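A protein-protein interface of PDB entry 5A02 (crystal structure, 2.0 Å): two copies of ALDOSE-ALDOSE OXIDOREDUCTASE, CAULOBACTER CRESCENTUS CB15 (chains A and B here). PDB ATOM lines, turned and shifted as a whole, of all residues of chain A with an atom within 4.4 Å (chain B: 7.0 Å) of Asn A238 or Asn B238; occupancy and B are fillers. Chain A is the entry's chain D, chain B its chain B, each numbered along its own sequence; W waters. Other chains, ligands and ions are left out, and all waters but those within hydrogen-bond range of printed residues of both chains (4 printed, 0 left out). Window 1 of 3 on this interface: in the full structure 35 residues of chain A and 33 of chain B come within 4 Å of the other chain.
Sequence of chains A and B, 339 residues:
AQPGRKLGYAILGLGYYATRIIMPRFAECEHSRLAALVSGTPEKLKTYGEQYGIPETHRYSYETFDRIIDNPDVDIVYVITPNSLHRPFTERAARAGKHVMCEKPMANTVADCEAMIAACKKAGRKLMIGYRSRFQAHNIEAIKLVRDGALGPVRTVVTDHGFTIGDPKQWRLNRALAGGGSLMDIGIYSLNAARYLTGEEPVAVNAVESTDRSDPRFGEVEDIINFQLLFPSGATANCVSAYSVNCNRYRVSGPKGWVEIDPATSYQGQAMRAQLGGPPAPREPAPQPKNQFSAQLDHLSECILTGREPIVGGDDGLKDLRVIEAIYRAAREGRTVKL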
ATOM      1  N   VAL A 157     -11.105 -17.377   8.054  1.00  0.00           N
ATOM      2  CA  VAL A 157     -10.821 -15.952   8.065  1.00  0.00           C
ATOM      3  C   VAL A 157     -10.336 -15.628   9.456  1.00  0.00           C
ATOM      4  O   VAL A 157     -11.058 -15.857  10.431  1.00  0.00           O
ATOM      5  CB  VAL A 157     -12.066 -15.066   7.737  1.00  0.00           C
ATOM      6  CG1 VAL A 157     -11.714 -13.576   7.894  1.00  0.00           C
ATOM      7  CG2 VAL A 157     -12.593 -15.336   6.334  1.00  0.00           C
ATOM      8  N   VAL A 158      -9.121 -15.107   9.570  1.00  0.00           N
ATOM      9  CA  VAL A 158      -8.606 -14.696  10.873  1.00  0.00           C
ATOM     10  C   VAL A 158      -8.418 -13.184  10.828  1.00  0.00           C
ATOM     11  O   VAL A 158      -7.635 -12.669  10.014  1.00  0.00           O
ATOM     12  CB  VAL A 158      -7.273 -15.428  11.228  1.00  0.00           C
ATOM     13  CG1 VAL A 158      -6.661 -14.871  12.534  1.00  0.00           C
ATOM     14  CG2 VAL A 158      -7.520 -16.924  11.352  1.00  0.00           C
ATOM     15  N   THR A 159      -9.167 -12.464  11.659  1.00  0.00           N
ATOM     16  CA  THR A 159      -9.182 -11.005  11.544  1.00  0.00           C
ATOM     17  C   THR A 159      -9.230 -10.351  12.922  1.00  0.00           C
ATOM     18  O   THR A 159     -10.018 -10.750  13.781  1.00  0.00           O
ATOM     19  CB  THR A 159     -10.376 -10.518  10.656  1.00  0.00           C
ATOM     20  OG1 THR A 159     -10.387  -9.083  10.590  1.00  0.00           O
ATOM     21  CG2 THR A 159     -11.743 -11.028  11.176  1.00  0.00           C
ATOM     22  N   ASN A 226     -13.878 -11.568  21.836  1.00  0.00           N
ATOM     23  CA  ASN A 226     -13.395 -12.290  20.663  1.00  0.00           C
ATOM     24  C   ASN A 226     -14.461 -13.278  20.250  1.00  0.00           C
ATOM     25  O   ASN A 226     -15.157 -13.798  21.116  1.00  0.00           O
ATOM     26  CB  ASN A 226     -12.088 -13.006  20.969  1.00  0.00           C
ATOM     27  CG  ASN A 226     -10.976 -12.049  21.342  1.00  0.00           C
ATOM     28  OD1 ASN A 226     -10.976 -10.887  20.926  1.00  0.00           O
ATOM     29  ND2 ASN A 226     -10.026 -12.529  22.142  1.00  0.00           N
ATOM     30  N   PHE A 227     -14.607 -13.542  18.952  1.00  0.00           N
ATOM     31  CA  PHE A 227     -15.699 -14.405  18.533  1.00  0.00           C
ATOM     32  C   PHE A 227     -15.332 -15.306  17.366  1.00  0.00           C
ATOM     33  O   PHE A 227     -14.396 -15.033  16.610  1.00  0.00           O
ATOM     34  CB  PHE A 227     -16.962 -13.574  18.199  1.00  0.00           C
ATOM     35  CG  PHE A 227     -16.736 -12.426  17.241  1.00  0.00           C
ATOM     36  CD1 PHE A 227     -16.237 -11.211  17.696  1.00  0.00           C
ATOM     37  CD2 PHE A 227     -17.055 -12.553  15.895  1.00  0.00           C
ATOM     38  CE1 PHE A 227     -16.035 -10.142  16.815  1.00  0.00           C
ATOM     39  CE2 PHE A 227     -16.884 -11.484  15.008  1.00  0.00           C
ATOM     40  CZ  PHE A 227     -16.370 -10.277  15.470  1.00  0.00           C
ATOM     41  N   GLN A 228     -16.057 -16.416  17.280  1.00  0.00           N
ATOM     42  CA  GLN A 228     -15.914 -17.391  16.212  1.00  0.00           C
ATOM     43  C   GLN A 228     -17.196 -17.422  15.422  1.00  0.00           C
ATOM     44  O   GLN A 228     -18.285 -17.365  16.002  1.00  0.00           O
ATOM     45  CB  GLN A 228     -15.628 -18.794  16.763  1.00  0.00           C
ATOM     46  CG  GLN A 228     -14.487 -18.867  17.734  1.00  0.00           C
ATOM     47  CD  GLN A 228     -14.210 -20.298  18.142  1.00  0.00           C
ATOM     48  OE1 GLN A 228     -15.010 -20.924  18.851  1.00  0.00           O
ATOM     49  NE2 GLN A 228     -13.090 -20.839  17.669  1.00  0.00           N
ATOM     50  N   ALA A 237     -14.510 -18.315  10.896  1.00  0.00           N
ATOM     51  CA  ALA A 237     -13.738 -17.116  11.217  1.00  0.00           C
ATOM     52  C   ALA A 237     -13.426 -17.053  12.703  1.00  0.00           C
ATOM     53  O   ALA A 237     -14.270 -17.389  13.532  1.00  0.00           O
ATOM     54  CB  ALA A 237     -14.487 -15.844  10.778  1.00  0.00           C
ATOM     55  N   ASN A 238     -12.191 -16.661  13.010  1.00  0.00           N
ATOM     56  CA  ASN A 238     -11.742 -16.311  14.355  1.00  0.00           C
ATOM     57  C   ASN A 238     -11.573 -14.814  14.370  1.00  0.00           C
ATOM     58  O   ASN A 238     -10.789 -14.291  13.585  1.00  0.00           O
ATOM     59  CB  ASN A 238     -10.406 -16.977  14.705  1.00  0.00           C
ATOM     60  CG  ASN A 238     -10.566 -18.332  15.367  1.00  0.00           C
ATOM     61  OD1 ASN A 238     -11.674 -18.809  15.587  1.00  0.00           O
ATOM     62  ND2 ASN A 238      -9.441 -18.958  15.692  1.00  0.00           N
ATOM     63  N   CYS A 239     -12.273 -14.113  15.254  1.00  0.00           N
ATOM     64  CA  CYS A 239     -12.227 -12.655  15.223  1.00  0.00           C
ATOM     65  C   CYS A 239     -11.840 -12.051  16.561  1.00  0.00           C
ATOM     66  O   CYS A 239     -12.304 -12.498  17.614  1.00  0.00           O
ATOM     67  CB  CYS A 239     -13.585 -12.090  14.789  1.00  0.00           C
ATOM     68  SG  CYS A 239     -14.218 -12.778  13.238  1.00  0.00           S
ATOM     69  N   VAL A 240     -10.993 -11.028  16.514  1.00  0.00           N
ATOM     70  CA  VAL A 240     -10.660 -10.249  17.703  1.00  0.00           C
ATOM     71  C   VAL A 240     -11.294  -8.868  17.623  1.00  0.00           C
ATOM     72  O   VAL A 240     -11.294  -8.225  16.567  1.00  0.00           O
ATOM     73  CB  VAL A 240      -9.128 -10.110  17.892  1.00  0.00           C
ATOM     74  CG1 VAL A 240      -8.785  -8.943  18.830  1.00  0.00           C
ATOM     75  CG2 VAL A 240      -8.533 -11.401  18.431  1.00  0.00           C
ATOM     76  N   THR B 156      -4.137 -10.574  24.087  1.00  0.00           N
ATOM     77  CA  THR B 156      -4.532 -11.516  23.038  1.00  0.00           C
ATOM     78  C   THR B 156      -3.357 -12.334  22.502  1.00  0.00           C
ATOM     79  O   THR B 156      -2.229 -11.840  22.374  1.00  0.00           O
ATOM     80  CB  THR B 156      -5.201 -10.805  21.831  1.00  0.00           C
ATOM     81  OG1 THR B 156      -4.251  -9.945  21.184  1.00  0.00           O
ATOM     82  CG2 THR B 156      -6.443 -10.000  22.260  1.00  0.00           C
ATOM     83  N   VAL B 157      -3.637 -13.598  22.203  1.00  0.00           N
ATOM     84  CA  VAL B 157      -2.748 -14.425  21.406  1.00  0.00           C
ATOM     85  C   VAL B 157      -3.557 -14.938  20.226  1.00  0.00           C
ATOM     86  O   VAL B 157      -4.601 -15.564  20.395  1.00  0.00           O
ATOM     87  CB  VAL B 157      -2.160 -15.612  22.202  1.00  0.00           C
ATOM     88  CG1 VAL B 157      -1.404 -16.550  21.267  1.00  0.00           C
ATOM     89  CG2 VAL B 157      -1.230 -15.111  23.324  1.00  0.00           C
ATOM     90  N   VAL B 158      -3.092 -14.651  19.024  1.00  0.00           N
ATOM     91  CA  VAL B 158      -3.797 -15.101  17.838  1.00  0.00           C
ATOM     92  C   VAL B 158      -2.815 -15.982  17.085  1.00  0.00           C
ATOM     93  O   VAL B 158      -1.778 -15.512  16.616  1.00  0.00           O
ATOM     94  CB  VAL B 158      -4.290 -13.914  16.978  1.00  0.00           C
ATOM     95  CG1 VAL B 158      -4.952 -14.404  15.679  1.00  0.00           C
ATOM     96  CG2 VAL B 158      -5.268 -13.041  17.784  1.00  0.00           C
ATOM     97  N   THR B 159      -3.130 -17.268  16.997  1.00  0.00           N
ATOM     98  CA  THR B 159      -2.176 -18.232  16.481  1.00  0.00           C
ATOM     99  C   THR B 159      -2.880 -19.243  15.585  1.00  0.00           C
ATOM    100  O   THR B 159      -3.943 -19.768  15.928  1.00  0.00           O
ATOM    101  CB  THR B 159      -1.420 -18.947  17.635  1.00  0.00           C
ATOM    102  OG1 THR B 159      -0.524 -19.926  17.098  1.00  0.00           O
ATOM    103  CG2 THR B 159      -2.380 -19.598  18.641  1.00  0.00           C
ATOM    104  N   ASP B 160      -2.303 -19.472  14.409  1.00  0.00           N
ATOM    105  CA  ASP B 160      -2.886 -20.375  13.414  1.00  0.00           C
ATOM    106  C   ASP B 160      -1.868 -21.437  13.025  1.00  0.00           C
ATOM    107  O   ASP B 160      -0.760 -21.095  12.595  1.00  0.00           O
ATOM    108  CB  ASP B 160      -3.300 -19.624  12.137  1.00  0.00           C
ATOM    109  CG  ASP B 160      -4.167 -18.404  12.406  1.00  0.00           C
ATOM    110  OD1 ASP B 160      -4.921 -18.382  13.404  1.00  0.00           O
ATOM    111  OD2 ASP B 160      -4.102 -17.462  11.582  1.00  0.00           O
ATOM    112  N   SER B 190      -0.630 -24.416  18.210  1.00  0.00           N
ATOM    113  CA  SER B 190      -1.360 -23.214  18.609  1.00  0.00           C
ATOM    114  C   SER B 190      -1.661 -23.247  20.106  1.00  0.00           C
ATOM    115  O   SER B 190      -1.482 -22.250  20.810  1.00  0.00           O
ATOM    116  CB  SER B 190      -2.674 -23.075  17.825  1.00  0.00           C
ATOM    117  OG  SER B 190      -2.447 -22.928  16.433  1.00  0.00           O
ATOM    118  N   ALA B 194      -0.015 -20.765  22.912  1.00  0.00           N
ATOM    119  CA  ALA B 194      -0.865 -19.908  23.749  1.00  0.00           C
ATOM    120  C   ALA B 194      -0.482 -20.081  25.216  1.00  0.00           C
ATOM    121  O   ALA B 194      -0.413 -19.115  25.978  1.00  0.00           O
ATOM    122  CB  ALA B 194      -2.345 -20.226  23.530  1.00  0.00           C
ATOM    123  N   VAL B 208     -15.185 -24.600  17.570  1.00  0.00           N
ATOM    124  CA  VAL B 208     -16.084 -24.941  16.490  1.00  0.00           C
ATOM    125  C   VAL B 208     -15.344 -25.867  15.524  1.00  0.00           C
ATOM    126  O   VAL B 208     -14.204 -25.589  15.112  1.00  0.00           O
ATOM    127  CB  VAL B 208     -16.619 -23.675  15.761  1.00  0.00           C
ATOM    128  CG1 VAL B 208     -15.498 -22.734  15.403  1.00  0.00           C
ATOM    129  CG2 VAL B 208     -17.407 -24.059  14.521  1.00  0.00           C
ATOM    130  N   ASN B 226     -11.332 -24.846  15.361  1.00  0.00           N
ATOM    131  CA  ASN B 226     -10.767 -23.604  15.874  1.00  0.00           C
ATOM    132  C   ASN B 226     -11.243 -23.395  17.281  1.00  0.00           C
ATOM    133  O   ASN B 226     -12.357 -23.790  17.618  1.00  0.00           O
ATOM    134  CB  ASN B 226     -11.168 -22.417  15.005  1.00  0.00           C
ATOM    135  CG  ASN B 226     -10.725 -22.576  13.573  1.00  0.00           C
ATOM    136  OD1 ASN B 226      -9.677 -23.167  13.300  1.00  0.00           O
ATOM    137  ND2 ASN B 226     -11.510 -22.039  12.648  1.00  0.00           N
ATOM    138  N   PHE B 227     -10.420 -22.782  18.120  1.00  0.00           N
ATOM    139  CA  PHE B 227     -10.807 -22.689  19.515  1.00  0.00           C
ATOM    140  C   PHE B 227     -10.381 -21.390  20.173  1.00  0.00           C
ATOM    141  O   PHE B 227      -9.439 -20.736  19.725  1.00  0.00           O
ATOM    142  CB  PHE B 227     -10.260 -23.899  20.300  1.00  0.00           C
ATOM    143  CG  PHE B 227      -8.768 -24.152  20.131  1.00  0.00           C
ATOM    144  CD1 PHE B 227      -8.275 -24.844  19.014  1.00  0.00           C
ATOM    145  CD2 PHE B 227      -7.873 -23.765  21.121  1.00  0.00           C
ATOM    146  CE1 PHE B 227      -6.903 -25.111  18.878  1.00  0.00           C
ATOM    147  CE2 PHE B 227      -6.505 -24.020  20.999  1.00  0.00           C
ATOM    148  CZ  PHE B 227      -6.019 -24.692  19.869  1.00  0.00           C
ATOM    149  N   GLN B 228     -11.106 -21.032  21.232  1.00  0.00           N
ATOM    150  CA  GLN B 228     -10.827 -19.847  22.048  1.00  0.00           C
ATOM    151  C   GLN B 228     -10.445 -20.265  23.445  1.00  0.00           C
ATOM    152  O   GLN B 228     -11.054 -21.186  24.010  1.00  0.00           O
ATOM    153  CB  GLN B 228     -12.045 -18.928  22.134  1.00  0.00           C
ATOM    154  CG  GLN B 228     -12.643 -18.543  20.810  1.00  0.00           C
ATOM    155  CD  GLN B 228     -13.770 -17.530  20.968  1.00  0.00           C
ATOM    156  OE1 GLN B 228     -14.829 -17.839  21.529  1.00  0.00           O
ATOM    157  NE2 GLN B 228     -13.545 -16.310  20.485  1.00  0.00           N
ATOM    158  N   LEU B 229      -9.457 -19.578  24.013  1.00  0.00           N
ATOM    159  CA  LEU B 229      -9.028 -19.833  25.380  1.00  0.00           C
ATOM    160  C   LEU B 229      -9.129 -18.558  26.196  1.00  0.00           C
ATOM    161  O   LEU B 229      -8.779 -17.477  25.724  1.00  0.00           O
ATOM    162  CB  LEU B 229      -7.584 -20.352  25.428  1.00  0.00           C
ATOM    163  CG  LEU B 229      -7.259 -21.576  24.568  1.00  0.00           C
ATOM    164  CD1 LEU B 229      -5.754 -21.892  24.622  1.00  0.00           C
ATOM    165  CD2 LEU B 229      -8.102 -22.774  25.004  1.00  0.00           C
ATOM    166  N   THR B 236      -6.535 -13.691  26.515  1.00  0.00           N
ATOM    167  CA  THR B 236      -7.345 -14.479  25.598  1.00  0.00           C
ATOM    168  C   THR B 236      -6.507 -15.037  24.448  1.00  0.00           C
ATOM    169  O   THR B 236      -5.479 -14.459  24.068  1.00  0.00           O
ATOM    170  CB  THR B 236      -8.505 -13.642  25.006  1.00  0.00           C
ATOM    171  OG1 THR B 236      -7.972 -12.572  24.217  1.00  0.00           O
ATOM    172  CG2 THR B 236      -9.396 -13.050  26.121  1.00  0.00           C
ATOM    173  N   ALA B 237      -6.954 -16.154  23.885  1.00  0.00           N
ATOM    174  CA  ALA B 237      -6.350 -16.679  22.658  1.00  0.00           C
ATOM    175  C   ALA B 237      -7.415 -17.093  21.657  1.00  0.00           C
ATOM    176  O   ALA B 237      -8.408 -17.721  22.041  1.00  0.00           O
ATOM    177  CB  ALA B 237      -5.440 -17.863  22.966  1.00  0.00           C
ATOM    178  N   ASN B 238      -7.205 -16.715  20.393  1.00  0.00           N
ATOM    179  CA  ASN B 238      -7.953 -17.225  19.241  1.00  0.00           C
ATOM    180  C   ASN B 238      -7.023 -18.148  18.467  1.00  0.00           C
ATOM    181  O   ASN B 238      -5.962 -17.706  18.019  1.00  0.00           O
ATOM    182  CB  ASN B 238      -8.423 -16.101  18.318  1.00  0.00           C
ATOM    183  CG  ASN B 238      -9.818 -15.585  18.645  1.00  0.00           C
ATOM    184  OD1 ASN B 238     -10.442 -15.999  19.619  1.00  0.00           O
ATOM    185  ND2 ASN B 238     -10.307 -14.652  17.819  1.00  0.00           N
ATOM    186  N   CYS B 239      -7.412 -19.410  18.302  1.00  0.00           N
ATOM    187  CA  CYS B 239      -6.523 -20.407  17.700  1.00  0.00           C
ATOM    188  C   CYS B 239      -7.144 -21.138  16.524  1.00  0.00           C
ATOM    189  O   CYS B 239      -8.291 -21.595  16.592  1.00  0.00           O
ATOM    190  CB  CYS B 239      -6.095 -21.455  18.731  1.00  0.00           C
ATOM    191  SG  CYS B 239      -5.395 -20.784  20.271  1.00  0.00           S
ATOM    192  N   VAL B 240      -6.364 -21.290  15.461  1.00  0.00           N
ATOM    193  CA  VAL B 240      -6.804 -22.099  14.325  1.00  0.00           C
ATOM    194  C   VAL B 240      -6.058 -23.419  14.324  1.00  0.00           C
ATOM    195  O   VAL B 240      -4.858 -23.465  14.625  1.00  0.00           O
ATOM    196  CB  VAL B 240      -6.595 -21.359  12.972  1.00  0.00           C
ATOM    197  CG1 VAL B 240      -6.613 -22.339  11.805  1.00  0.00           C
ATOM    198  CG2 VAL B 240      -7.683 -20.332  12.780  1.00  0.00           C
ATOM    199  N   SER B 241      -6.786 -24.494  14.035  1.00  0.00           N
ATOM    200  CA  SER B 241      -6.198 -25.798  13.781  1.00  0.00           C
ATOM    201  C   SER B 241      -6.830 -26.347  12.502  1.00  0.00           C
ATOM    202  O   SER B 241      -8.052 -26.470  12.429  1.00  0.00           O
ATOM    203  CB  SER B 241      -6.440 -26.739  14.961  1.00  0.00           C
ATOM    204  OG  SER B 241      -5.961 -28.040  14.687  1.00  0.00           O
HETATM  205  O   HOH W   1     -13.591 -20.199  14.004  1.00  0.00           O
HETATM  206  O   HOH W   2      -6.910 -17.706  15.164  1.00  0.00           O
HETATM  207  O   HOH W   3     -10.346 -15.548  22.404  1.00  0.00           O
HETATM  208  O   HOH W   4      -8.604 -13.736  15.613  1.00  0.00           O
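The backbone carbonyl oxygen (O) of Val B157 is in hydrogen-bond range of the backbone NH (N) of Asn B238, at 2.8 Å.
O of Asn B238 lies within hydrogen-bond range of N of Thr B159.
O of Asn B226 sits at hydrogen-bond distance from N of Val B208 (2.9 Å).
The backbone carbonyl oxygen (O) of Phe B227 sits at hydrogen-bond distance from the backbone NH (N) of Cys B239, at 2.8 Å.
O of Asn A238 lies within hydrogen-bond range of N of Thr A159.
N of Val A240 lies within hydrogen-bond range of O of Thr A159 (2.9 Å).
Val A158 touches its own counterpart, Val B158.
Val A158 touches Val B240, and with the chains exchanged Val A240 touches Val B158.
Phe A227 touches Gln B228, and with the chains exchanged Gln A228 touches Phe B227.
Asn A238 touches Val B240, and with the chains exchanged Val A240 touches Asn B238.
Of the 18 pairs that touch across the chains among the printed residues, 15 have their exchanged pair printed and touching as well.
Of the 18 printed residues of chain B, 10 touch a printed residue of chain A.
Hydrophobic or aromatic side chains of chain B within 4 Å of the printed part of chain A: Val B158, Val B208 and Val B240.
Of the 10 printed residues of chain A, 7 touch a printed residue of chain B.
Hydrophobic or aromatic side chains of chain A that line the printed part of chain B: Val A158 and Val A240.
Among the printed residues, 18 pairs touch across the chains.
Asn A238 touches just these residues of chain B: Asn B226 (3.7 Å), Asn B238 (3.7 Å), Cys B239 (3.0 Å) and Val B240 (3.7 Å).
Of the printed residues of chain B, Cys A239 touches Asn B238 (2.9 Å).
Printed residues of chain B within 4 Å of Val A240: Val B158 (3.7 Å) and Asn B238 (3.8 Å).
Of the printed residues of chain A, Asp B160 touches Val A158 (3.5 Å).
Of the printed residues of chain A, Thr B236 touches Asn A226 (2.9 Å).
Asn B238 touches just these residues of chain A: Asn A226 (3.7 Å), Asn A238 (3.7 Å), Cys A239 (2.9 Å) and Val A240 (3.8 Å).
Of the printed residues of chain A, Val B240 touches Val A158 and Asn A238.
Ser B241 touches none of the printed residues of chain A.
The nearest residue of chain B that does not touch Asn A238 is Phe B227 (4.4 Å).
Val A158 touches Val B158.
Asp B160 touches Val A158 (OD2 to CG2, 3.5 Å).
CG2 of Val B240 touches CG2 of Val A158, 3.7 Å away.
Asn A226 touches Asn B238 (CB to OD1, 3.7 Å).
NE2 of Gln A228 touches CG1 of Val B208, at 3.8 Å.
Asn B226 touches Asn A238 (CB to OD1, 3.7 Å).
Asn A238 touches Asn B238 (C to ND2, 3.7 Å).
Asn A238 touches Val B240.
CG2 of Val A240 touches CG2 of Val B158, at 3.7 Å.
Asn B238 touches Val A240.
NE2 of Gln A228 lies within hydrogen-bond range of O of Asn B226, 3.0 Å away.
N of Phe B227 sits close to NE2 of Gln A228 (3.3 Å).
The side-chain amide nitrogen (NE2) of Gln B228 lies within hydrogen-bond range of the backbone carbonyl oxygen (O) of Asn A226 (3.1 Å).
The side-chain amide nitrogen (NE2) of Gln B228 lies close to the backbone NH (N) of Phe A227 (3.3 Å).
The side-chain amide nitrogen (ND2) of Asn A226 lies within hydrogen-bond range of the side-chain hydroxyl (OG1) of Thr B236, 2.9 Å away.
ND2 of Asn B238 sits at hydrogen-bond distance from O of Cys A239 (2.9 Å).
ND2 of Asn A238 is in hydrogen-bond range of O of Cys B239.
Water W2 lies within hydrogen-bond range of OD1 of Asp B160 (2.7 Å), ND2 of Asn A238 (2.9 Å) and O of Asn B238 (3.0 Å).
Water W3 lies within hydrogen-bond range of the side-chain amide oxygen of Asn B238, the backbone carbonyl oxygen of Ala B237 and the side-chain amide nitrogen of Asn A226.
Water W1 lies within hydrogen-bond range of the side-chain amide oxygen of Asn A238 (2.8 Å), the backbone carbonyl oxygen of Ala A237 (2.9 Å) and the side-chain amide nitrogen of Asn B226 (3.1 Å).
Water W4 lies within hydrogen-bond range of the side-chain amide nitrogen of Asn B238 (2.9 Å) and the backbone carbonyl oxygen of Asn A238 (3.0 Å).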
